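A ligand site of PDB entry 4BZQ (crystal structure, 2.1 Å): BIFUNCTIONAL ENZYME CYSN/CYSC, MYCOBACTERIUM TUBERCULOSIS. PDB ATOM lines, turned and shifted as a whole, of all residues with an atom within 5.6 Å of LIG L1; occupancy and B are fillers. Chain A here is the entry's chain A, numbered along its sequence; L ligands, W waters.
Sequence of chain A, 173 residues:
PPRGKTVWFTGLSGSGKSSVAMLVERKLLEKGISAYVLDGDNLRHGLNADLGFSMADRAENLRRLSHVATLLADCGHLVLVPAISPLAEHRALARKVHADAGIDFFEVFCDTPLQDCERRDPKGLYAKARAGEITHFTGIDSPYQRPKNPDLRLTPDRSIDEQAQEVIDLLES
The guanidinium group of Arg 44 lies within hydrogen-bond range of the backbone carbonyl oxygen of Gly 52, at 2.8 Å. The guanidinium group (NH2) of Arg 58 is in hydrogen-bond range of the backbone carbonyl oxygen (O) of His 136 (2.9 Å). The guanidinium group (NE) of Arg 58 is in hydrogen-bond range of the backbone carbonyl oxygen (O) of Phe 53 (2.8 Å). NH1 of Arg 58 sits at hydrogen-bond distance from OG1 of Thr 138 (2.9 Å). The side-chain hydroxyl (OG) of Ser 85 sits at hydrogen-bond distance from the backbone carbonyl oxygen (O) of Ala 83. N of Gly 40 lies within hydrogen-bond range of O of Pro 82, 3.0 Å away.
Ser 13 touches LIG L1 (OG to O9, 3.9 Å). Gly 40 touches LIG L1. Phe 53 touches LIG L1 (CE2 to N2, 3.3 Å). Leu 62 touches LIG L1. Ala 83 touches LIG L1. Pro 86 touches LIG L1. Leu 125 touches LIG L1. O of Thr 135 touches N3 of LIG L1, 3.8 Å away. Phe 137 touches LIG L1. N of Thr 138 touches N4 of LIG L1 (3.6 Å). Hydrophobic or aromatic side chains that line LIG L1: Phe 53, Leu 62, Ala 83, Ile 84, Pro 86, Leu 125 and Phe 137. Within 4 Å of LIG L1: Ser 13, Gly 40, Asp 41, Arg 44, Phe 53, Arg 58, Asn 61, Leu 62, Ala 83, Ile 84, Ser 85, Pro 86, Lys 123, Leu 125, Thr 135, His 136, Phe 137 and Thr 138.
Water W2 lies within hydrogen-bond range of O9 of LIG L1 (2.5 Å), NZ of Lys 17 (2.8 Å) and O1 of LG2 L2 (3.1 Å). Water W1 bridges the backbone carbonyl oxygen of Thr 135 (2.6 Å) and a nitrogen (N3) of LIG L1 (2.9 Å).
The side-chain amino group of Lys 123 sits at hydrogen-bond distance from an oxygen (O10) of LIG L1, 2.6 Å away. The guanidinium group (NH2) of Arg 44 is in salt-bridge range of an oxygen (O3) of LIG L1, at 2.8 Å. An oxygen (O2) of LIG L1 lies within salt-bridge range of the guanidinium group (NH1) of Arg 58, at 2.9 Å. The side-chain carboxylate (OD1) of Asp 41 lies within hydrogen-bond range of an oxygen (O10) of LIG L1 (2.9 Å). The backbone NH of Ile 84 sits at hydrogen-bond distance from an oxygen (O5) of LIG L1 (2.9 Å). ND2 of Asn 61 is in hydrogen-bond range of O4 of LIG L1 (2.9 Å). The backbone NH (N) of Ser 85 sits at hydrogen-bond distance from an oxygen (O1) of LIG L1 (2.9 Å). The backbone carbonyl oxygen (O) of His 136 lies within hydrogen-bond range of a nitrogen (N3) of LIG L1. The backbone NH of Lys 17 is in hydrogen-bond range of an oxygen (O2) of LG2 L2 (2.8 Å). NZ of Lys 17 lies within salt-bridge range of O2 of LG2 L2 (2.8 Å). The backbone NH (N) of Gly 14 is in hydrogen-bond range of an oxygen (O1) of LG2 L2, at 2.8 Å.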
ATOM      1  N   SER A  13       8.556 -29.928   7.690  1.00  0.00           N
ATOM      2  CA  SER A  13       8.394 -30.062   9.094  1.00  0.00           C
ATOM      3  C   SER A  13       7.757 -31.409   9.407  1.00  0.00           C
ATOM      4  O   SER A  13       6.820 -31.839   8.729  1.00  0.00           O
ATOM      5  CB  SER A  13       7.559 -28.911   9.590  1.00  0.00           C
ATOM      6  OG  SER A  13       7.399 -28.964  10.989  1.00  0.00           O
ATOM      7  N   GLY A  14       8.320 -32.096  10.395  1.00  0.00           N
ATOM      8  CA  GLY A  14       7.867 -33.411  10.761  1.00  0.00           C
ATOM      9  C   GLY A  14       8.261 -34.563   9.833  1.00  0.00           C
ATOM     10  O   GLY A  14       7.667 -35.656   9.892  1.00  0.00           O
ATOM     11  N   LYS A  17      13.827 -35.014  10.315  1.00  0.00           N
ATOM     12  CA  LYS A  17      15.205 -34.452  10.204  1.00  0.00           C
ATOM     13  C   LYS A  17      15.958 -34.518  11.525  1.00  0.00           C
ATOM     14  O   LYS A  17      17.061 -35.094  11.600  1.00  0.00           O
ATOM     15  CB  LYS A  17      15.196 -33.017   9.708  1.00  0.00           C
ATOM     16  CG  LYS A  17      14.546 -32.844   8.357  1.00  0.00           C
ATOM     17  CD  LYS A  17      14.564 -31.418   7.883  1.00  0.00           C
ATOM     18  CE  LYS A  17      13.822 -30.453   8.789  1.00  0.00           C
ATOM     19  NZ  LYS A  17      12.369 -30.721   8.728  1.00  0.00           N
ATOM     20  N   GLY A  40      18.150 -26.485  13.535  1.00  0.00           N
ATOM     21  CA  GLY A  40      17.525 -25.221  13.094  1.00  0.00           C
ATOM     22  C   GLY A  40      16.598 -24.634  14.134  1.00  0.00           C
ATOM     23  O   GLY A  40      16.746 -23.450  14.532  1.00  0.00           O
ATOM     24  N   ASP A  41      15.710 -25.500  14.632  1.00  0.00           N
ATOM     25  CA  ASP A  41      14.759 -25.123  15.665  1.00  0.00           C
ATOM     26  C   ASP A  41      15.423 -24.691  16.991  1.00  0.00           C
ATOM     27  O   ASP A  41      15.041 -23.671  17.551  1.00  0.00           O
ATOM     28  CB  ASP A  41      13.769 -26.256  15.930  1.00  0.00           C
ATOM     29  CG  ASP A  41      12.486 -25.764  16.538  1.00  0.00           C
ATOM     30  OD1 ASP A  41      11.637 -25.225  15.802  1.00  0.00           O
ATOM     31  OD2 ASP A  41      12.320 -25.882  17.777  1.00  0.00           O
ATOM     32  N   ARG A  44      17.319 -21.415  16.614  1.00  0.00           N
ATOM     33  CA  ARG A  44      16.357 -20.311  16.512  1.00  0.00           C
ATOM     34  C   ARG A  44      16.013 -19.730  17.878  1.00  0.00           C
ATOM     35  O   ARG A  44      15.517 -18.665  17.931  1.00  0.00           O
ATOM     36  CB  ARG A  44      15.100 -20.693  15.719  1.00  0.00           C
ATOM     37  CG  ARG A  44      15.377 -20.634  14.221  1.00  0.00           C
ATOM     38  CD  ARG A  44      14.179 -21.100  13.405  1.00  0.00           C
ATOM     39  NE  ARG A  44      14.300 -20.854  11.964  1.00  0.00           N
ATOM     40  CZ  ARG A  44      14.010 -19.713  11.357  1.00  0.00           C
ATOM     41  NH1 ARG A  44      13.595 -18.660  12.075  1.00  0.00           N
ATOM     42  NH2 ARG A  44      14.118 -19.590  10.024  1.00  0.00           N
ATOM     43  N   GLY A  52      12.734 -14.693  11.861  1.00  0.00           N
ATOM     44  CA  GLY A  52      11.442 -15.368  11.692  1.00  0.00           C
ATOM     45  C   GLY A  52      11.429 -16.270  10.469  1.00  0.00           C
ATOM     46  O   GLY A  52      12.439 -16.945  10.158  1.00  0.00           O
ATOM     47  N   PHE A  53      10.269 -16.320   9.794  1.00  0.00           N
ATOM     48  CA  PHE A  53      10.068 -17.282   8.701  1.00  0.00           C
ATOM     49  C   PHE A  53       9.763 -16.665   7.352  1.00  0.00           C
ATOM     50  O   PHE A  53       9.467 -17.389   6.412  1.00  0.00           O
ATOM     51  CB  PHE A  53       9.042 -18.337   9.078  1.00  0.00           C
ATOM     52  CG  PHE A  53       9.483 -19.165  10.263  1.00  0.00           C
ATOM     53  CD1 PHE A  53      10.367 -20.228  10.083  1.00  0.00           C
ATOM     54  CD2 PHE A  53       9.097 -18.809  11.587  1.00  0.00           C
ATOM     55  CE1 PHE A  53      10.827 -20.963  11.171  1.00  0.00           C
ATOM     56  CE2 PHE A  53       9.576 -19.539  12.654  1.00  0.00           C
ATOM     57  CZ  PHE A  53      10.417 -20.617  12.457  1.00  0.00           C
ATOM     58  N   ASP A  57      14.543 -14.116   6.131  1.00  0.00           N
ATOM     59  CA  ASP A  57      15.056 -14.585   7.391  1.00  0.00           C
ATOM     60  C   ASP A  57      15.473 -16.050   7.329  1.00  0.00           C
ATOM     61  O   ASP A  57      16.510 -16.437   7.903  1.00  0.00           O
ATOM     62  CB  ASP A  57      13.975 -14.453   8.491  1.00  0.00           C
ATOM     63  CG  ASP A  57      13.806 -13.010   8.996  1.00  0.00           C
ATOM     64  OD1 ASP A  57      14.526 -12.123   8.476  1.00  0.00           O
ATOM     65  OD2 ASP A  57      12.979 -12.771   9.929  1.00  0.00           O
ATOM     66  N   ARG A  58      14.701 -16.894   6.613  1.00  0.00           N
ATOM     67  CA  ARG A  58      15.104 -18.247   6.441  1.00  0.00           C
ATOM     68  C   ARG A  58      16.450 -18.313   5.712  1.00  0.00           C
ATOM     69  O   ARG A  58      17.326 -19.110   6.102  1.00  0.00           O
ATOM     70  CB  ARG A  58      14.076 -19.038   5.655  1.00  0.00           C
ATOM     71  CG  ARG A  58      12.754 -19.213   6.374  1.00  0.00           C
ATOM     72  CD  ARG A  58      11.830 -19.921   5.416  1.00  0.00           C
ATOM     73  NE  ARG A  58      10.427 -19.960   5.804  1.00  0.00           N
ATOM     74  CZ  ARG A  58       9.776 -21.025   6.259  1.00  0.00           C
ATOM     75  NH1 ARG A  58      10.397 -22.174   6.547  1.00  0.00           N
ATOM     76  NH2 ARG A  58       8.484 -20.893   6.477  1.00  0.00           N
ATOM     77  N   ASN A  61      19.092 -17.332   8.245  1.00  0.00           N
ATOM     78  CA  ASN A  61      19.179 -18.398   9.183  1.00  0.00           C
ATOM     79  C   ASN A  61      20.077 -19.498   8.632  1.00  0.00           C
ATOM     80  O   ASN A  61      21.062 -19.858   9.235  1.00  0.00           O
ATOM     81  CB  ASN A  61      17.789 -18.935   9.428  1.00  0.00           C
ATOM     82  CG  ASN A  61      17.758 -20.128  10.377  1.00  0.00           C
ATOM     83  OD1 ASN A  61      18.120 -20.005  11.540  1.00  0.00           O
ATOM     84  ND2 ASN A  61      17.262 -21.279   9.904  1.00  0.00           N
ATOM     85  N   LEU A  62      19.729 -19.947   7.440  1.00  0.00           N
ATOM     86  CA  LEU A  62      20.478 -20.989   6.796  1.00  0.00           C
ATOM     87  C   LEU A  62      21.913 -20.552   6.373  1.00  0.00           C
ATOM     88  O   LEU A  62      22.862 -21.350   6.457  1.00  0.00           O
ATOM     89  CB  LEU A  62      19.688 -21.503   5.623  1.00  0.00           C
ATOM     90  CG  LEU A  62      18.330 -22.094   6.050  1.00  0.00           C
ATOM     91  CD1 LEU A  62      17.465 -22.327   4.853  1.00  0.00           C
ATOM     92  CD2 LEU A  62      18.481 -23.324   6.962  1.00  0.00           C
ATOM     93  N   LEU A  65      23.816 -20.715   9.633  1.00  0.00           N
ATOM     94  CA  LEU A  65      24.064 -22.100   9.919  1.00  0.00           C
ATOM     95  C   LEU A  65      25.133 -22.710   9.058  1.00  0.00           C
ATOM     96  O   LEU A  65      25.927 -23.502   9.541  1.00  0.00           O
ATOM     97  CB  LEU A  65      22.793 -22.932   9.784  1.00  0.00           C
ATOM     98  CG  LEU A  65      21.700 -22.769  10.826  1.00  0.00           C
ATOM     99  CD1 LEU A  65      20.567 -23.747  10.490  1.00  0.00           C
ATOM    100  CD2 LEU A  65      22.327 -23.096  12.144  1.00  0.00           C
ATOM    101  N   PRO A  82      19.898 -30.505  10.670  1.00  0.00           N
ATOM    102  CA  PRO A  82      18.522 -30.608  10.307  1.00  0.00           C
ATOM    103  C   PRO A  82      17.877 -29.249  10.314  1.00  0.00           C
ATOM    104  O   PRO A  82      17.787 -28.602  11.391  1.00  0.00           O
ATOM    105  CB  PRO A  82      17.903 -31.423  11.436  1.00  0.00           C
ATOM    106  CG  PRO A  82      18.718 -31.013  12.633  1.00  0.00           C
ATOM    107  CD  PRO A  82      20.089 -30.740  12.136  1.00  0.00           C
ATOM    108  N   ALA A  83      17.465 -28.820   9.150  1.00  0.00           N
ATOM    109  CA  ALA A  83      16.761 -27.585   8.987  1.00  0.00           C
ATOM    110  C   ALA A  83      15.960 -27.725   7.707  1.00  0.00           C
ATOM    111  O   ALA A  83      16.417 -28.350   6.764  1.00  0.00           O
ATOM    112  CB  ALA A  83      17.759 -26.455   8.852  1.00  0.00           C
ATOM    113  N   ILE A  84      14.788 -27.133   7.669  1.00  0.00           N
ATOM    114  CA  ILE A  84      13.895 -27.339   6.550  1.00  0.00           C
ATOM    115  C   ILE A  84      14.547 -27.046   5.221  1.00  0.00           C
ATOM    116  O   ILE A  84      14.431 -27.849   4.274  1.00  0.00           O
ATOM    117  CB  ILE A  84      12.635 -26.476   6.693  1.00  0.00           C
ATOM    118  CG1 ILE A  84      11.830 -27.076   7.872  1.00  0.00           C
ATOM    119  CG2 ILE A  84      11.864 -26.496   5.361  1.00  0.00           C
ATOM    120  CD1 ILE A  84      10.557 -26.347   8.218  1.00  0.00           C
ATOM    121  N   SER A  85      15.232 -25.910   5.160  1.00  0.00           N
ATOM    122  CA  SER A  85      15.917 -25.506   3.903  1.00  0.00           C
ATOM    123  C   SER A  85      14.970 -25.568   2.689  1.00  0.00           C
ATOM    124  O   SER A  85      15.195 -26.333   1.747  1.00  0.00           O
ATOM    125  CB  SER A  85      17.137 -26.398   3.674  1.00  0.00           C
ATOM    126  OG  SER A  85      17.985 -26.370   4.803  1.00  0.00           O
ATOM    127  N   PRO A  86      13.885 -24.818   2.730  1.00  0.00           N
ATOM    128  CA  PRO A  86      12.770 -25.080   1.779  1.00  0.00           C
ATOM    129  C   PRO A  86      13.051 -24.761   0.283  1.00  0.00           C
ATOM    130  O   PRO A  86      12.445 -25.375  -0.595  1.00  0.00           O
ATOM    131  CB  PRO A  86      11.621 -24.224   2.341  1.00  0.00           C
ATOM    132  CG  PRO A  86      12.311 -23.087   3.043  1.00  0.00           C
ATOM    133  CD  PRO A  86      13.540 -23.754   3.680  1.00  0.00           C
ATOM    134  N   HIS A  90      18.594 -22.139  -1.103  1.00  0.00           N
ATOM    135  CA  HIS A  90      19.072 -22.314   0.270  1.00  0.00           C
ATOM    136  C   HIS A  90      20.095 -23.432   0.354  1.00  0.00           C
ATOM    137  O   HIS A  90      21.184 -23.254   0.900  1.00  0.00           O
ATOM    138  CB  HIS A  90      17.912 -22.641   1.207  1.00  0.00           C
ATOM    139  CG  HIS A  90      16.938 -21.547   1.341  1.00  0.00           C
ATOM    140  ND1 HIS A  90      15.685 -21.734   1.885  1.00  0.00           N
ATOM    141  CD2 HIS A  90      17.034 -20.227   1.035  1.00  0.00           C
ATOM    142  CE1 HIS A  90      15.048 -20.574   1.916  1.00  0.00           C
ATOM    143  NE2 HIS A  90      15.864 -19.631   1.442  1.00  0.00           N
ATOM    144  N   LYS A 123       4.308 -31.487  16.786  1.00  0.00           N
ATOM    145  CA  LYS A 123       4.208 -30.282  17.624  1.00  0.00           C
ATOM    146  C   LYS A 123       2.887 -29.522  17.410  1.00  0.00           C
ATOM    147  O   LYS A 123       2.746 -28.368  17.852  1.00  0.00           O
ATOM    148  CB  LYS A 123       5.331 -29.316  17.300  1.00  0.00           C
ATOM    149  CG  LYS A 123       6.759 -29.833  17.453  1.00  0.00           C
ATOM    150  CD  LYS A 123       7.628 -29.276  16.336  1.00  0.00           C
ATOM    151  CE  LYS A 123       9.111 -29.420  16.595  1.00  0.00           C
ATOM    152  NZ  LYS A 123       9.823 -28.858  15.431  1.00  0.00           N
ATOM    153  N   LEU A 125       1.718 -28.241  14.736  1.00  0.00           N
ATOM    154  CA  LEU A 125       1.865 -27.031  13.924  1.00  0.00           C
ATOM    155  C   LEU A 125       1.041 -27.056  12.639  1.00  0.00           C
ATOM    156  O   LEU A 125       0.595 -26.017  12.166  1.00  0.00           O
ATOM    157  CB  LEU A 125       3.317 -26.787  13.578  1.00  0.00           C
ATOM    158  CG  LEU A 125       4.267 -26.388  14.729  1.00  0.00           C
ATOM    159  CD1 LEU A 125       5.699 -26.349  14.202  1.00  0.00           C
ATOM    160  CD2 LEU A 125       3.932 -25.050  15.345  1.00  0.00           C
ATOM    161  N   ILE A 134      -1.165 -20.054  12.345  1.00  0.00           N
ATOM    162  CA  ILE A 134       0.174 -19.741  11.899  1.00  0.00           C
ATOM    163  C   ILE A 134       0.075 -19.516  10.404  1.00  0.00           C
ATOM    164  O   ILE A 134      -0.719 -20.186   9.752  1.00  0.00           O
ATOM    165  CB  ILE A 134       1.147 -20.926  12.128  1.00  0.00           C
ATOM    166  CG1 ILE A 134       1.251 -21.221  13.610  1.00  0.00           C
ATOM    167  CG2 ILE A 134       2.541 -20.643  11.586  1.00  0.00           C
ATOM    168  CD1 ILE A 134       1.897 -22.550  13.902  1.00  0.00           C
ATOM    169  N   THR A 135       0.895 -18.611   9.869  1.00  0.00           N
ATOM    170  CA  THR A 135       0.945 -18.373   8.443  1.00  0.00           C
ATOM    171  C   THR A 135       2.367 -18.558   7.946  1.00  0.00           C
ATOM    172  O   THR A 135       3.331 -18.562   8.717  1.00  0.00           O
ATOM    173  CB  THR A 135       0.443 -16.954   8.072  1.00  0.00           C
ATOM    174  OG1 THR A 135       1.272 -15.982   8.707  1.00  0.00           O
ATOM    175  CG2 THR A 135      -0.989 -16.759   8.549  1.00  0.00           C
ATOM    176  N   HIS A 136       2.479 -18.690   6.634  1.00  0.00           N
ATOM    177  CA  HIS A 136       3.751 -18.924   5.959  1.00  0.00           C
ATOM    178  C   HIS A 136       4.406 -20.211   6.449  1.00  0.00           C
ATOM    179  O   HIS A 136       5.601 -20.299   6.611  1.00  0.00           O
ATOM    180  CB  HIS A 136       4.685 -17.687   6.110  1.00  0.00           C
ATOM    181  CG  HIS A 136       4.172 -16.471   5.400  1.00  0.00           C
ATOM    182  ND1 HIS A 136       3.611 -15.405   6.070  1.00  0.00           N
ATOM    183  CD2 HIS A 136       4.088 -16.178   4.087  1.00  0.00           C
ATOM    184  CE1 HIS A 136       3.243 -14.487   5.196  1.00  0.00           C
ATOM    185  NE2 HIS A 136       3.509 -14.938   3.986  1.00  0.00           N
ATOM    186  N   PHE A 137       3.587 -21.210   6.685  1.00  0.00           N
ATOM    187  CA  PHE A 137       4.071 -22.486   7.133  1.00  0.00           C
ATOM    188  C   PHE A 137       4.414 -23.377   5.949  1.00  0.00           C
ATOM    189  O   PHE A 137       3.546 -23.688   5.088  1.00  0.00           O
ATOM    190  CB  PHE A 137       3.031 -23.166   8.035  1.00  0.00           C
ATOM    191  CG  PHE A 137       3.612 -24.282   8.818  1.00  0.00           C
ATOM    192  CD1 PHE A 137       4.365 -24.012   9.963  1.00  0.00           C
ATOM    193  CD2 PHE A 137       3.472 -25.600   8.407  1.00  0.00           C
ATOM    194  CE1 PHE A 137       4.949 -25.036  10.678  1.00  0.00           C
ATOM    195  CE2 PHE A 137       4.035 -26.615   9.146  1.00  0.00           C
ATOM    196  CZ  PHE A 137       4.791 -26.340  10.267  1.00  0.00           C
ATOM    197  N   THR A 138       5.661 -23.816   5.930  1.00  0.00           N
ATOM    198  CA  THR A 138       6.209 -24.647   4.852  1.00  0.00           C
ATOM    199  C   THR A 138       5.301 -25.809   4.467  1.00  0.00           C
ATOM    200  O   THR A 138       4.815 -26.543   5.338  1.00  0.00           O
ATOM    201  CB  THR A 138       7.647 -25.172   5.206  1.00  0.00           C
ATOM    202  OG1 THR A 138       8.562 -24.056   5.419  1.00  0.00           O
ATOM    203  CG2 THR A 138       8.219 -26.036   4.045  1.00  0.00           C
HETATM  204  S1  LIG L   1      14.167 -22.917   7.766  1.00  0.00           S
HETATM  205  O1  LIG L   1      15.188 -23.854   7.275  1.00  0.00           O
HETATM  206  O2  LIG L   1      13.218 -22.680   6.683  1.00  0.00           O
HETATM  207  O3  LIG L   1      14.762 -21.610   8.178  1.00  0.00           O
HETATM  208  P1  LIG L   1      14.155 -24.105  10.294  1.00  0.00           P
HETATM  209  O4  LIG L   1      15.290 -23.244  10.754  1.00  0.00           O
HETATM  210  O5  LIG L   1      14.482 -25.545  10.059  1.00  0.00           O
HETATM  211  O6  LIG L   1      13.437 -23.354   9.029  1.00  0.00           O
HETATM  212  O7  LIG L   1      13.070 -24.034  11.444  1.00  0.00           O
HETATM  213  C1  LIG L   1      11.849 -24.726  11.238  1.00  0.00           C
HETATM  214  C2  LIG L   1      11.239 -25.203  12.531  1.00  0.00           C
HETATM  215  O8  LIG L   1      10.524 -24.102  13.069  1.00  0.00           O
HETATM  216  C3  LIG L   1      10.197 -26.290  12.305  1.00  0.00           C
HETATM  217  O9  LIG L   1      10.665 -27.620  12.573  1.00  0.00           O
HETATM  218  C4  LIG L   1       9.057 -25.879  13.202  1.00  0.00           C
HETATM  219  O10 LIG L   1       9.420 -26.448  14.438  1.00  0.00           O
HETATM  220  C5  LIG L   1       9.176 -24.418  13.493  1.00  0.00           C
HETATM  221  N1  LIG L   1       8.337 -23.471  12.746  1.00  0.00           N
HETATM  222  C6  LIG L   1       7.725 -22.434  13.321  1.00  0.00           C
HETATM  223  N2  LIG L   1       7.086 -21.679  12.405  1.00  0.00           N
HETATM  224  C7  LIG L   1       7.360 -22.212  11.208  1.00  0.00           C
HETATM  225  C8  LIG L   1       6.980 -21.883   9.827  1.00  0.00           C
HETATM  226  N3  LIG L   1       6.191 -20.812   9.655  1.00  0.00           N
HETATM  227  N4  LIG L   1       7.435 -22.638   8.808  1.00  0.00           N
HETATM  228  C9  LIG L   1       8.172 -23.733   9.078  1.00  0.00           C
HETATM  229  N5  LIG L   1       8.547 -24.109  10.332  1.00  0.00           N
HETATM  230  C10 LIG L   1       8.185 -23.379  11.403  1.00  0.00           C
HETATM  231  P1  LG2 L   2      11.676 -32.639  11.728  1.00  0.00           P
HETATM  232  O1  LG2 L   2      10.597 -31.667  12.011  1.00  0.00           O
HETATM  233  O2  LG2 L   2      11.914 -33.036  10.299  1.00  0.00           O
HETATM  234  O3  LG2 L   2      12.922 -32.405  12.571  1.00  0.00           O
HETATM  235  P2  LG2 L   2      11.157 -34.739  13.586  1.00  0.00           P
HETATM  236  O4  LG2 L   2      10.954 -33.806  14.714  1.00  0.00           O
HETATM  237  O5  LG2 L   2      12.327 -35.658  13.442  1.00  0.00           O
HETATM  238  O6  LG2 L   2      10.931 -33.958  12.198  1.00  0.00           O
HETATM  239  O7  LG2 L   2       9.794 -35.486  13.650  1.00  0.00           O
HETATM  240  C1  LG2 L   2       9.448 -36.473  12.749  1.00  0.00           C
HETATM  241  C2  LG2 L   2       8.393 -37.275  13.495  1.00  0.00           C
HETATM  242  O8  LG2 L   2       8.061 -38.458  12.791  1.00  0.00           O
HETATM  243  C3  LG2 L   2       8.957 -37.735  14.804  1.00  0.00           C
HETATM  244  O9  LG2 L   2       7.950 -37.650  15.794  1.00  0.00           O
HETATM  245  C4  LG2 L   2       9.294 -39.179  14.632  1.00  0.00           C
HETATM  246  O10 LG2 L   2       8.615 -39.747  15.728  1.00  0.00           O
HETATM  247  C5  LG2 L   2       8.615 -39.627  13.385  1.00  0.00           C
HETATM  248  N1  LG2 L   2       9.482 -40.269  12.386  1.00  0.00           N
HETATM  249  C6  LG2 L   2      10.399 -39.695  11.579  1.00  0.00           C
HETATM  250  N2  LG2 L   2      10.965 -40.593  10.708  1.00  0.00           N
HETATM  251  C7  LG2 L   2      10.398 -41.773  11.004  1.00  0.00           C
HETATM  252  C8  LG2 L   2      10.509 -43.159  10.516  1.00  0.00           C
HETATM  253  N3  LG2 L   2      11.390 -43.429   9.542  1.00  0.00           N
HETATM  254  N4  LG2 L   2       9.730 -44.106  11.064  1.00  0.00           N
HETATM  255  C9  LG2 L   2       8.865 -43.830  12.054  1.00  0.00           C
HETATM  256  N5  LG2 L   2       8.720 -42.591  12.542  1.00  0.00           N
HETATM  257  C10 LG2 L   2       9.427 -41.556  12.074  1.00  0.00           C
HETATM  258  O   HOH W   1       5.368 -18.121  10.295  1.00  0.00           O
HETATM  259  O   HOH W   2      11.484 -29.035  10.724  1.00  0.00           O
